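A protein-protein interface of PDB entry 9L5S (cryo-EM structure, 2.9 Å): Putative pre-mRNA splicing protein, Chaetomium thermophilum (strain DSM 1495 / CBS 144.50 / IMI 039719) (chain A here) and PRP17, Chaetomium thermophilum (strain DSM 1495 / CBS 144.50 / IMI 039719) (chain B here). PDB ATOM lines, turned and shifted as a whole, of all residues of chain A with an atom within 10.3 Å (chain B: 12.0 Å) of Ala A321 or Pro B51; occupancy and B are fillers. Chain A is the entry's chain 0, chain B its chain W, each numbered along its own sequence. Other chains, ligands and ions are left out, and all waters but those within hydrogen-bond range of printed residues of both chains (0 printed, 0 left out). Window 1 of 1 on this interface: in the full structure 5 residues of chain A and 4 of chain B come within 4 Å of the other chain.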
ATOM      1  N   PHE A 281       5.399  10.424 -23.714  1.00  0.00           N
ATOM      2  CA  PHE A 281       5.815  11.823 -23.758  1.00  0.00           C
ATOM      3  C   PHE A 281       4.744  12.690 -24.408  1.00  0.00           C
ATOM      4  O   PHE A 281       4.311  13.696 -23.836  1.00  0.00           O
ATOM      5  CB  PHE A 281       7.129  11.956 -24.530  1.00  0.00           C
ATOM      6  CG  PHE A 281       8.358  11.631 -23.724  1.00  0.00           C
ATOM      7  CD1 PHE A 281       8.266  11.044 -22.470  1.00  0.00           C
ATOM      8  CD2 PHE A 281       9.615  11.913 -24.233  1.00  0.00           C
ATOM      9  CE1 PHE A 281       9.404  10.743 -21.749  1.00  0.00           C
ATOM     10  CE2 PHE A 281      10.753  11.617 -23.516  1.00  0.00           C
ATOM     11  CZ  PHE A 281      10.650  11.029 -22.277  1.00  0.00           C
ATOM     12  N   TYR A 302      10.074  14.705  -8.340  1.00  0.00           N
ATOM     13  CA  TYR A 302      11.451  14.271  -8.077  1.00  0.00           C
ATOM     14  C   TYR A 302      11.880  14.542  -6.636  1.00  0.00           C
ATOM     15  O   TYR A 302      13.029  14.909  -6.378  1.00  0.00           O
ATOM     16  CB  TYR A 302      12.434  14.914  -9.060  1.00  0.00           C
ATOM     17  CG  TYR A 302      12.265  14.464 -10.493  1.00  0.00           C
ATOM     18  CD1 TYR A 302      12.799  13.260 -10.934  1.00  0.00           C
ATOM     19  CD2 TYR A 302      11.566  15.246 -11.407  1.00  0.00           C
ATOM     20  CE1 TYR A 302      12.645  12.847 -12.245  1.00  0.00           C
ATOM     21  CE2 TYR A 302      11.406  14.841 -12.720  1.00  0.00           C
ATOM     22  CZ  TYR A 302      11.947  13.641 -13.133  1.00  0.00           C
ATOM     23  OH  TYR A 302      11.791  13.234 -14.438  1.00  0.00           O
ATOM     24  N   TYR A 307       7.315  21.668  -7.381  1.00  0.00           N
ATOM     25  CA  TYR A 307       8.260  21.935  -8.459  1.00  0.00           C
ATOM     26  C   TYR A 307       7.527  22.183  -9.777  1.00  0.00           C
ATOM     27  O   TYR A 307       7.611  23.282 -10.336  1.00  0.00           O
ATOM     28  CB  TYR A 307       9.238  20.761  -8.605  1.00  0.00           C
ATOM     29  CG  TYR A 307      10.372  20.971  -9.598  1.00  0.00           C
ATOM     30  CD1 TYR A 307      11.080  19.887 -10.098  1.00  0.00           C
ATOM     31  CD2 TYR A 307      10.774  22.248  -9.989  1.00  0.00           C
ATOM     32  CE1 TYR A 307      12.114  20.061 -10.997  1.00  0.00           C
ATOM     33  CE2 TYR A 307      11.807  22.430 -10.885  1.00  0.00           C
ATOM     34  CZ  TYR A 307      12.476  21.333 -11.383  1.00  0.00           C
ATOM     35  OH  TYR A 307      13.513  21.511 -12.270  1.00  0.00           O
ATOM     36  N   ALA A 309       8.165  20.475 -12.808  1.00  0.00           N
ATOM     37  CA  ALA A 309       9.368  20.491 -13.638  1.00  0.00           C
ATOM     38  C   ALA A 309       9.115  21.023 -15.045  1.00  0.00           C
ATOM     39  O   ALA A 309       8.078  20.720 -15.647  1.00  0.00           O
ATOM     40  CB  ALA A 309       9.961  19.083 -13.723  1.00  0.00           C
ATOM     41  N   PRO A 310      10.027  21.831 -15.585  1.00  0.00           N
ATOM     42  CA  PRO A 310       9.807  22.415 -16.912  1.00  0.00           C
ATOM     43  C   PRO A 310       9.865  21.367 -18.012  1.00  0.00           C
ATOM     44  O   PRO A 310      10.447  20.291 -17.852  1.00  0.00           O
ATOM     45  CB  PRO A 310      10.952  23.428 -17.052  1.00  0.00           C
ATOM     46  CG  PRO A 310      11.474  23.631 -15.658  1.00  0.00           C
ATOM     47  CD  PRO A 310      11.270  22.324 -14.971  1.00  0.00           C
ATOM     48  N   ASP A 311       9.232  21.699 -19.141  1.00  0.00           N
ATOM     49  CA  ASP A 311       9.180  20.793 -20.283  1.00  0.00           C
ATOM     50  C   ASP A 311      10.551  20.539 -20.896  1.00  0.00           C
ATOM     51  O   ASP A 311      10.744  19.501 -21.536  1.00  0.00           O
ATOM     52  CB  ASP A 311       8.229  21.348 -21.343  1.00  0.00           C
ATOM     53  CG  ASP A 311       6.872  21.706 -20.776  1.00  0.00           C
ATOM     54  OD1 ASP A 311       6.491  21.127 -19.736  1.00  0.00           O
ATOM     55  OD2 ASP A 311       6.187  22.568 -21.365  1.00  0.00           O
ATOM     56  N   ALA A 312      11.498  21.465 -20.729  1.00  0.00           N
ATOM     57  CA  ALA A 312      12.862  21.214 -21.177  1.00  0.00           C
ATOM     58  C   ALA A 312      13.521  20.106 -20.367  1.00  0.00           C
ATOM     59  O   ALA A 312      14.268  19.293 -20.922  1.00  0.00           O
ATOM     60  CB  ALA A 312      13.688  22.497 -21.095  1.00  0.00           C
ATOM     61  N   VAL A 313      13.256  20.056 -19.065  1.00  0.00           N
ATOM     62  CA  VAL A 313      13.846  19.038 -18.203  1.00  0.00           C
ATOM     63  C   VAL A 313      13.049  17.740 -18.242  1.00  0.00           C
ATOM     64  O   VAL A 313      13.627  16.655 -18.347  1.00  0.00           O
ATOM     65  CB  VAL A 313      13.965  19.579 -16.765  1.00  0.00           C
ATOM     66  CG1 VAL A 313      14.656  18.565 -15.875  1.00  0.00           C
ATOM     67  CG2 VAL A 313      14.717  20.900 -16.757  1.00  0.00           C
ATOM     68  N   HIS A 314      11.720  17.827 -18.163  1.00  0.00           N
ATOM     69  CA  HIS A 314      10.897  16.622 -18.129  1.00  0.00           C
ATOM     70  C   HIS A 314      10.847  15.951 -19.497  1.00  0.00           C
ATOM     71  O   HIS A 314      11.246  14.792 -19.648  1.00  0.00           O
ATOM     72  CB  HIS A 314       9.489  16.961 -17.638  1.00  0.00           C
ATOM     73  CG  HIS A 314       8.639  15.758 -17.369  1.00  0.00           C
ATOM     74  ND1 HIS A 314       7.340  15.649 -17.817  1.00  0.00           N
ATOM     75  CD2 HIS A 314       8.904  14.611 -16.702  1.00  0.00           C
ATOM     76  CE1 HIS A 314       6.841  14.487 -17.436  1.00  0.00           C
ATOM     77  NE2 HIS A 314       7.770  13.838 -16.757  1.00  0.00           N
ATOM     78  N   PHE A 315      10.363  16.670 -20.512  1.00  0.00           N
ATOM     79  CA  PHE A 315      10.304  16.142 -21.875  1.00  0.00           C
ATOM     80  C   PHE A 315      11.674  16.297 -22.537  1.00  0.00           C
ATOM     81  O   PHE A 315      11.893  17.123 -23.425  1.00  0.00           O
ATOM     82  CB  PHE A 315       9.213  16.838 -22.677  1.00  0.00           C
ATOM     83  CG  PHE A 315       7.863  16.815 -22.020  1.00  0.00           C
ATOM     84  CD1 PHE A 315       7.358  15.642 -21.483  1.00  0.00           C
ATOM     85  CD2 PHE A 315       7.097  17.966 -21.943  1.00  0.00           C
ATOM     86  CE1 PHE A 315       6.114  15.618 -20.879  1.00  0.00           C
ATOM     87  CE2 PHE A 315       5.852  17.950 -21.340  1.00  0.00           C
ATOM     88  CZ  PHE A 315       5.361  16.775 -20.808  1.00  0.00           C
ATOM     89  N   ALA A 316      12.612  15.471 -22.079  1.00  0.00           N
ATOM     90  CA  ALA A 316      13.965  15.449 -22.608  1.00  0.00           C
ATOM     91  C   ALA A 316      14.355  14.014 -22.927  1.00  0.00           C
ATOM     92  O   ALA A 316      13.968  13.078 -22.223  1.00  0.00           O
ATOM     93  CB  ALA A 316      14.971  16.059 -21.623  1.00  0.00           C
ATOM     94  N   ARG A 317      15.124  13.850 -24.000  1.00  0.00           N
ATOM     95  CA  ARG A 317      15.558  12.538 -24.458  1.00  0.00           C
ATOM     96  C   ARG A 317      17.077  12.490 -24.488  1.00  0.00           C
ATOM     97  O   ARG A 317      17.718  13.369 -25.072  1.00  0.00           O
ATOM     98  CB  ARG A 317      14.986  12.221 -25.843  1.00  0.00           C
ATOM     99  CG  ARG A 317      13.516  11.842 -25.822  1.00  0.00           C
ATOM    100  CD  ARG A 317      13.070  11.263 -27.152  1.00  0.00           C
ATOM    101  NE  ARG A 317      13.189  12.235 -28.231  1.00  0.00           N
ATOM    102  CZ  ARG A 317      13.118  11.934 -29.520  1.00  0.00           C
ATOM    103  NH1 ARG A 317      12.928  10.691 -29.930  1.00  0.00           N
ATOM    104  NH2 ARG A 317      13.239  12.905 -30.421  1.00  0.00           N
ATOM    105  N   GLY A 318      17.644  11.469 -23.854  1.00  0.00           N
ATOM    106  CA  GLY A 318      19.074  11.286 -23.832  1.00  0.00           C
ATOM    107  C   GLY A 318      19.495  10.204 -22.859  1.00  0.00           C
ATOM    108  O   GLY A 318      18.688   9.686 -22.081  1.00  0.00           O
ATOM    109  N   PRO A 319      20.779   9.839 -22.887  1.00  0.00           N
ATOM    110  CA  PRO A 319      21.259   8.818 -21.946  1.00  0.00           C
ATOM    111  C   PRO A 319      21.383   9.325 -20.521  1.00  0.00           C
ATOM    112  O   PRO A 319      21.228   8.536 -19.582  1.00  0.00           O
ATOM    113  CB  PRO A 319      22.622   8.424 -22.529  1.00  0.00           C
ATOM    114  CG  PRO A 319      23.087   9.653 -23.235  1.00  0.00           C
ATOM    115  CD  PRO A 319      21.851  10.335 -23.768  1.00  0.00           C
ATOM    116  N   ASN A 320      21.657  10.614 -20.330  1.00  0.00           N
ATOM    117  CA  ASN A 320      21.884  11.181 -19.008  1.00  0.00           C
ATOM    118  C   ASN A 320      20.703  11.997 -18.494  1.00  0.00           C
ATOM    119  O   ASN A 320      20.834  12.676 -17.472  1.00  0.00           O
ATOM    120  CB  ASN A 320      23.148  12.039 -19.018  1.00  0.00           C
ATOM    121  CG  ASN A 320      23.236  12.933 -20.239  1.00  0.00           C
ATOM    122  OD1 ASN A 320      22.273  13.073 -20.992  1.00  0.00           O
ATOM    123  ND2 ASN A 320      24.395  13.550 -20.438  1.00  0.00           N
ATOM    124  N   ALA A 321      19.562  11.956 -19.178  1.00  0.00           N
ATOM    125  CA  ALA A 321      18.380  12.654 -18.701  1.00  0.00           C
ATOM    126  C   ALA A 321      17.817  11.959 -17.460  1.00  0.00           C
ATOM    127  O   ALA A 321      18.117  10.797 -17.176  1.00  0.00           O
ATOM    128  CB  ALA A 321      17.321  12.729 -19.799  1.00  0.00           C
ATOM    129  N   VAL A 322      16.992  12.685 -16.717  1.00  0.00           N
ATOM    130  CA  VAL A 322      16.351  12.156 -15.513  1.00  0.00           C
ATOM    131  C   VAL A 322      14.849  12.074 -15.788  1.00  0.00           C
ATOM    132  O   VAL A 322      14.065  12.998 -15.545  1.00  0.00           O
ATOM    133  CB  VAL A 322      16.702  12.966 -14.258  1.00  0.00           C
ATOM    134  CG1 VAL A 322      18.168  12.773 -13.947  1.00  0.00           C
ATOM    135  CG2 VAL A 322      16.531  14.469 -14.486  1.00  0.00           C
ATOM    136  N   ASN A 323      14.434  10.908 -16.286  1.00  0.00           N
ATOM    137  CA  ASN A 323      13.109  10.621 -16.815  1.00  0.00           C
ATOM    138  C   ASN A 323      13.217   9.133 -17.148  1.00  0.00           C
ATOM    139  O   ASN A 323      14.335   8.605 -17.136  1.00  0.00           O
ATOM    140  CB  ASN A 323      12.846  11.509 -18.043  1.00  0.00           C
ATOM    141  CG  ASN A 323      11.378  11.610 -18.440  1.00  0.00           C
ATOM    142  OD1 ASN A 323      10.494  11.022 -17.835  1.00  0.00           O
ATOM    143  ND2 ASN A 323      11.118  12.417 -19.458  1.00  0.00           N
ATOM    144  N   PRO A 324      12.124   8.404 -17.402  1.00  0.00           N
ATOM    145  CA  PRO A 324      12.247   7.104 -18.089  1.00  0.00           C
ATOM    146  C   PRO A 324      13.011   7.109 -19.424  1.00  0.00           C
ATOM    147  O   PRO A 324      13.303   6.014 -19.923  1.00  0.00           O
ATOM    148  CB  PRO A 324      10.786   6.698 -18.292  1.00  0.00           C
ATOM    149  CG  PRO A 324      10.099   7.249 -17.046  1.00  0.00           C
ATOM    150  CD  PRO A 324      11.003   8.333 -16.447  1.00  0.00           C
ATOM    151  N   ARG A 325      13.306   8.277 -20.012  1.00  0.00           N
ATOM    152  CA  ARG A 325      14.184   8.441 -21.171  1.00  0.00           C
ATOM    153  C   ARG A 325      13.654   7.713 -22.402  1.00  0.00           C
ATOM    154  O   ARG A 325      12.620   8.093 -22.960  1.00  0.00           O
ATOM    155  CB  ARG A 325      15.604   7.952 -20.855  1.00  0.00           C
ATOM    156  CG  ARG A 325      16.319   8.710 -19.750  1.00  0.00           C
ATOM    157  CD  ARG A 325      17.578   7.961 -19.316  1.00  0.00           C
ATOM    158  NE  ARG A 325      17.985   8.267 -17.948  1.00  0.00           N
ATOM    159  CZ  ARG A 325      17.390   7.802 -16.857  1.00  0.00           C
ATOM    160  NH1 ARG A 325      16.358   6.974 -16.928  1.00  0.00           N
ATOM    161  NH2 ARG A 325      17.845   8.169 -15.664  1.00  0.00           N
ATOM    162  N   GLY A 326      14.360   6.671 -22.827  1.00  0.00           N
ATOM    163  CA  GLY A 326      13.973   5.906 -23.998  1.00  0.00           C
ATOM    164  C   GLY A 326      15.016   4.881 -24.402  1.00  0.00           C
ATOM    165  O   GLY A 326      16.191   5.009 -24.057  1.00  0.00           O
ATOM    166  N   TYR B  46      34.959  15.704 -14.588  1.00  0.00           N
ATOM    167  CA  TYR B  46      34.207  15.929 -13.365  1.00  0.00           C
ATOM    168  C   TYR B  46      32.884  16.630 -13.662  1.00  0.00           C
ATOM    169  O   TYR B  46      32.599  17.037 -14.791  1.00  0.00           O
ATOM    170  CB  TYR B  46      35.013  16.775 -12.382  1.00  0.00           C
ATOM    171  CG  TYR B  46      36.049  16.010 -11.599  1.00  0.00           C
ATOM    172  CD1 TYR B  46      35.712  14.864 -10.895  1.00  0.00           C
ATOM    173  CD2 TYR B  46      37.369  16.444 -11.557  1.00  0.00           C
ATOM    174  CE1 TYR B  46      36.661  14.164 -10.179  1.00  0.00           C
ATOM    175  CE2 TYR B  46      38.326  15.753 -10.840  1.00  0.00           C
ATOM    176  CZ  TYR B  46      37.965  14.614 -10.151  1.00  0.00           C
ATOM    177  OH  TYR B  46      38.914  13.920  -9.436  1.00  0.00           O
ATOM    178  N   GLY B  47      32.072  16.769 -12.619  1.00  0.00           N
ATOM    179  CA  GLY B  47      30.849  17.525 -12.709  1.00  0.00           C
ATOM    180  C   GLY B  47      29.671  16.699 -13.177  1.00  0.00           C
ATOM    181  O   GLY B  47      29.808  15.539 -13.577  1.00  0.00           O
ATOM    182  N   PRO B  48      28.482  17.291 -13.131  1.00  0.00           N
ATOM    183  CA  PRO B  48      27.272  16.584 -13.557  1.00  0.00           C
ATOM    184  C   PRO B  48      27.193  16.466 -15.075  1.00  0.00           C
ATOM    185  O   PRO B  48      28.052  16.942 -15.816  1.00  0.00           O
ATOM    186  CB  PRO B  48      26.135  17.462 -13.017  1.00  0.00           C
ATOM    187  CG  PRO B  48      26.793  18.428 -12.068  1.00  0.00           C
ATOM    188  CD  PRO B  48      28.173  18.616 -12.577  1.00  0.00           C
ATOM    189  N   ALA B  49      26.129  15.813 -15.523  1.00  0.00           N
ATOM    190  CA  ALA B  49      25.874  15.637 -16.943  1.00  0.00           C
ATOM    191  C   ALA B  49      24.727  16.535 -17.399  1.00  0.00           C
ATOM    192  O   ALA B  49      23.833  16.886 -16.627  1.00  0.00           O
ATOM    193  CB  ALA B  49      25.557  14.175 -17.253  1.00  0.00           C
ATOM    194  N   ASN B  50      24.776  16.911 -18.674  1.00  0.00           N
ATOM    195  CA  ASN B  50      23.759  17.778 -19.258  1.00  0.00           C
ATOM    196  C   ASN B  50      22.443  17.017 -19.371  1.00  0.00           C
ATOM    197  O   ASN B  50      22.413  15.941 -19.978  1.00  0.00           O
ATOM    198  CB  ASN B  50      24.212  18.262 -20.634  1.00  0.00           C
ATOM    199  CG  ASN B  50      23.407  19.451 -21.147  1.00  0.00           C
ATOM    200  OD1 ASN B  50      22.177  19.451 -21.127  1.00  0.00           O
ATOM    201  ND2 ASN B  50      24.112  20.467 -21.628  1.00  0.00           N
ATOM    202  N   PRO B  51      21.342  17.529 -18.813  1.00  0.00           N
ATOM    203  CA  PRO B  51      20.057  16.826 -18.956  1.00  0.00           C
ATOM    204  C   PRO B  51      19.395  17.042 -20.305  1.00  0.00           C
ATOM    205  O   PRO B  51      18.377  16.396 -20.584  1.00  0.00           O
ATOM    206  CB  PRO B  51      19.197  17.408 -17.824  1.00  0.00           C
ATOM    207  CG  PRO B  51      20.107  18.268 -16.999  1.00  0.00           C
ATOM    208  CD  PRO B  51      21.267  18.643 -17.858  1.00  0.00           C
ATOM    209  N   PHE B  52      19.930  17.921 -21.147  1.00  0.00           N
ATOM    210  CA  PHE B  52      19.319  18.217 -22.436  1.00  0.00           C
ATOM    211  C   PHE B  52      20.118  17.602 -23.582  1.00  0.00           C
ATOM    212  O   PHE B  52      21.348  17.607 -23.568  1.00  0.00           O
ATOM    213  CB  PHE B  52      19.195  19.729 -22.632  1.00  0.00           C
ATOM    214  CG  PHE B  52      18.670  20.456 -21.427  1.00  0.00           C
ATOM    215  CD1 PHE B  52      17.334  20.365 -21.073  1.00  0.00           C
ATOM    216  CD2 PHE B  52      19.514  21.231 -20.647  1.00  0.00           C
ATOM    217  CE1 PHE B  52      16.849  21.032 -19.962  1.00  0.00           C
ATOM    218  CE2 PHE B  52      19.036  21.901 -19.536  1.00  0.00           C
ATOM    219  CZ  PHE B  52      17.701  21.802 -19.194  1.00  0.00           C
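The side-chain amide oxygen (OD1) of Asn A320 sits close to the backbone carbonyl oxygen (O) of Asn B50 (3.0 Å).
NE of Arg A325 is in hydrogen-bond range of O of Ala A321 (2.6 Å).
The side-chain amide oxygen of Asn B50 is in hydrogen-bond range of the backbone NH of Phe B52 (2.7 Å).
Among the printed residues, merely in contact across the chains: Ala A312 with Phe B52 (3.3 Å), Val A313 with Phe B52 (3.8 Å), Ala A316 with Pro B51 (3.6 Å), Asn A320 with Ala B49 (3.4 Å) and Ala A321 with Pro B51 (3.9 Å).
Printed residues of chain B within 4 Å of Ala A312: Phe B52.
Of chain B, only Phe B52 (3.8 Å) comes within 4 Å of Val A313.
Ala A316 touches one residue of chain B.
No residue of chain B comes within 4 Å of Pro A319.
Of chain B, only Pro B51 (3.9 Å) comes within 4 Å of Ala A321.
No residue of chain B comes within 4 Å of Asn A323.
No residue of chain B comes within 4 Å of Arg A325.
Of chain A, only Asn A320 comes within 4 Å of Asn B50.
Of chain A, only Ala A316 and Ala A321 come within 4 Å of Pro B51.
The nearest residue of chain B that does not touch Ala A321 is Asn B50 (5.0 Å).
The nearest residue of chain A that does not touch Pro B51 is Asn A320 (4.5 Å).
The nearest printed residue of chain B that does not touch Ala A312 is Pro B51 (5.0 Å).
Of the 21 printed residues of chain A, 5 touch a printed residue of chain B.
Hydrophobic or aromatic side chains of chain A that line the printed part of chain B: Ala A312, Val A313, Ala A316 and Ala A321.
Hydrophobic or aromatic side chains of chain B that line the printed part of chain A: Ala B49 and Phe B52.
Among the printed residues, 6 pairs touch across the chains.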
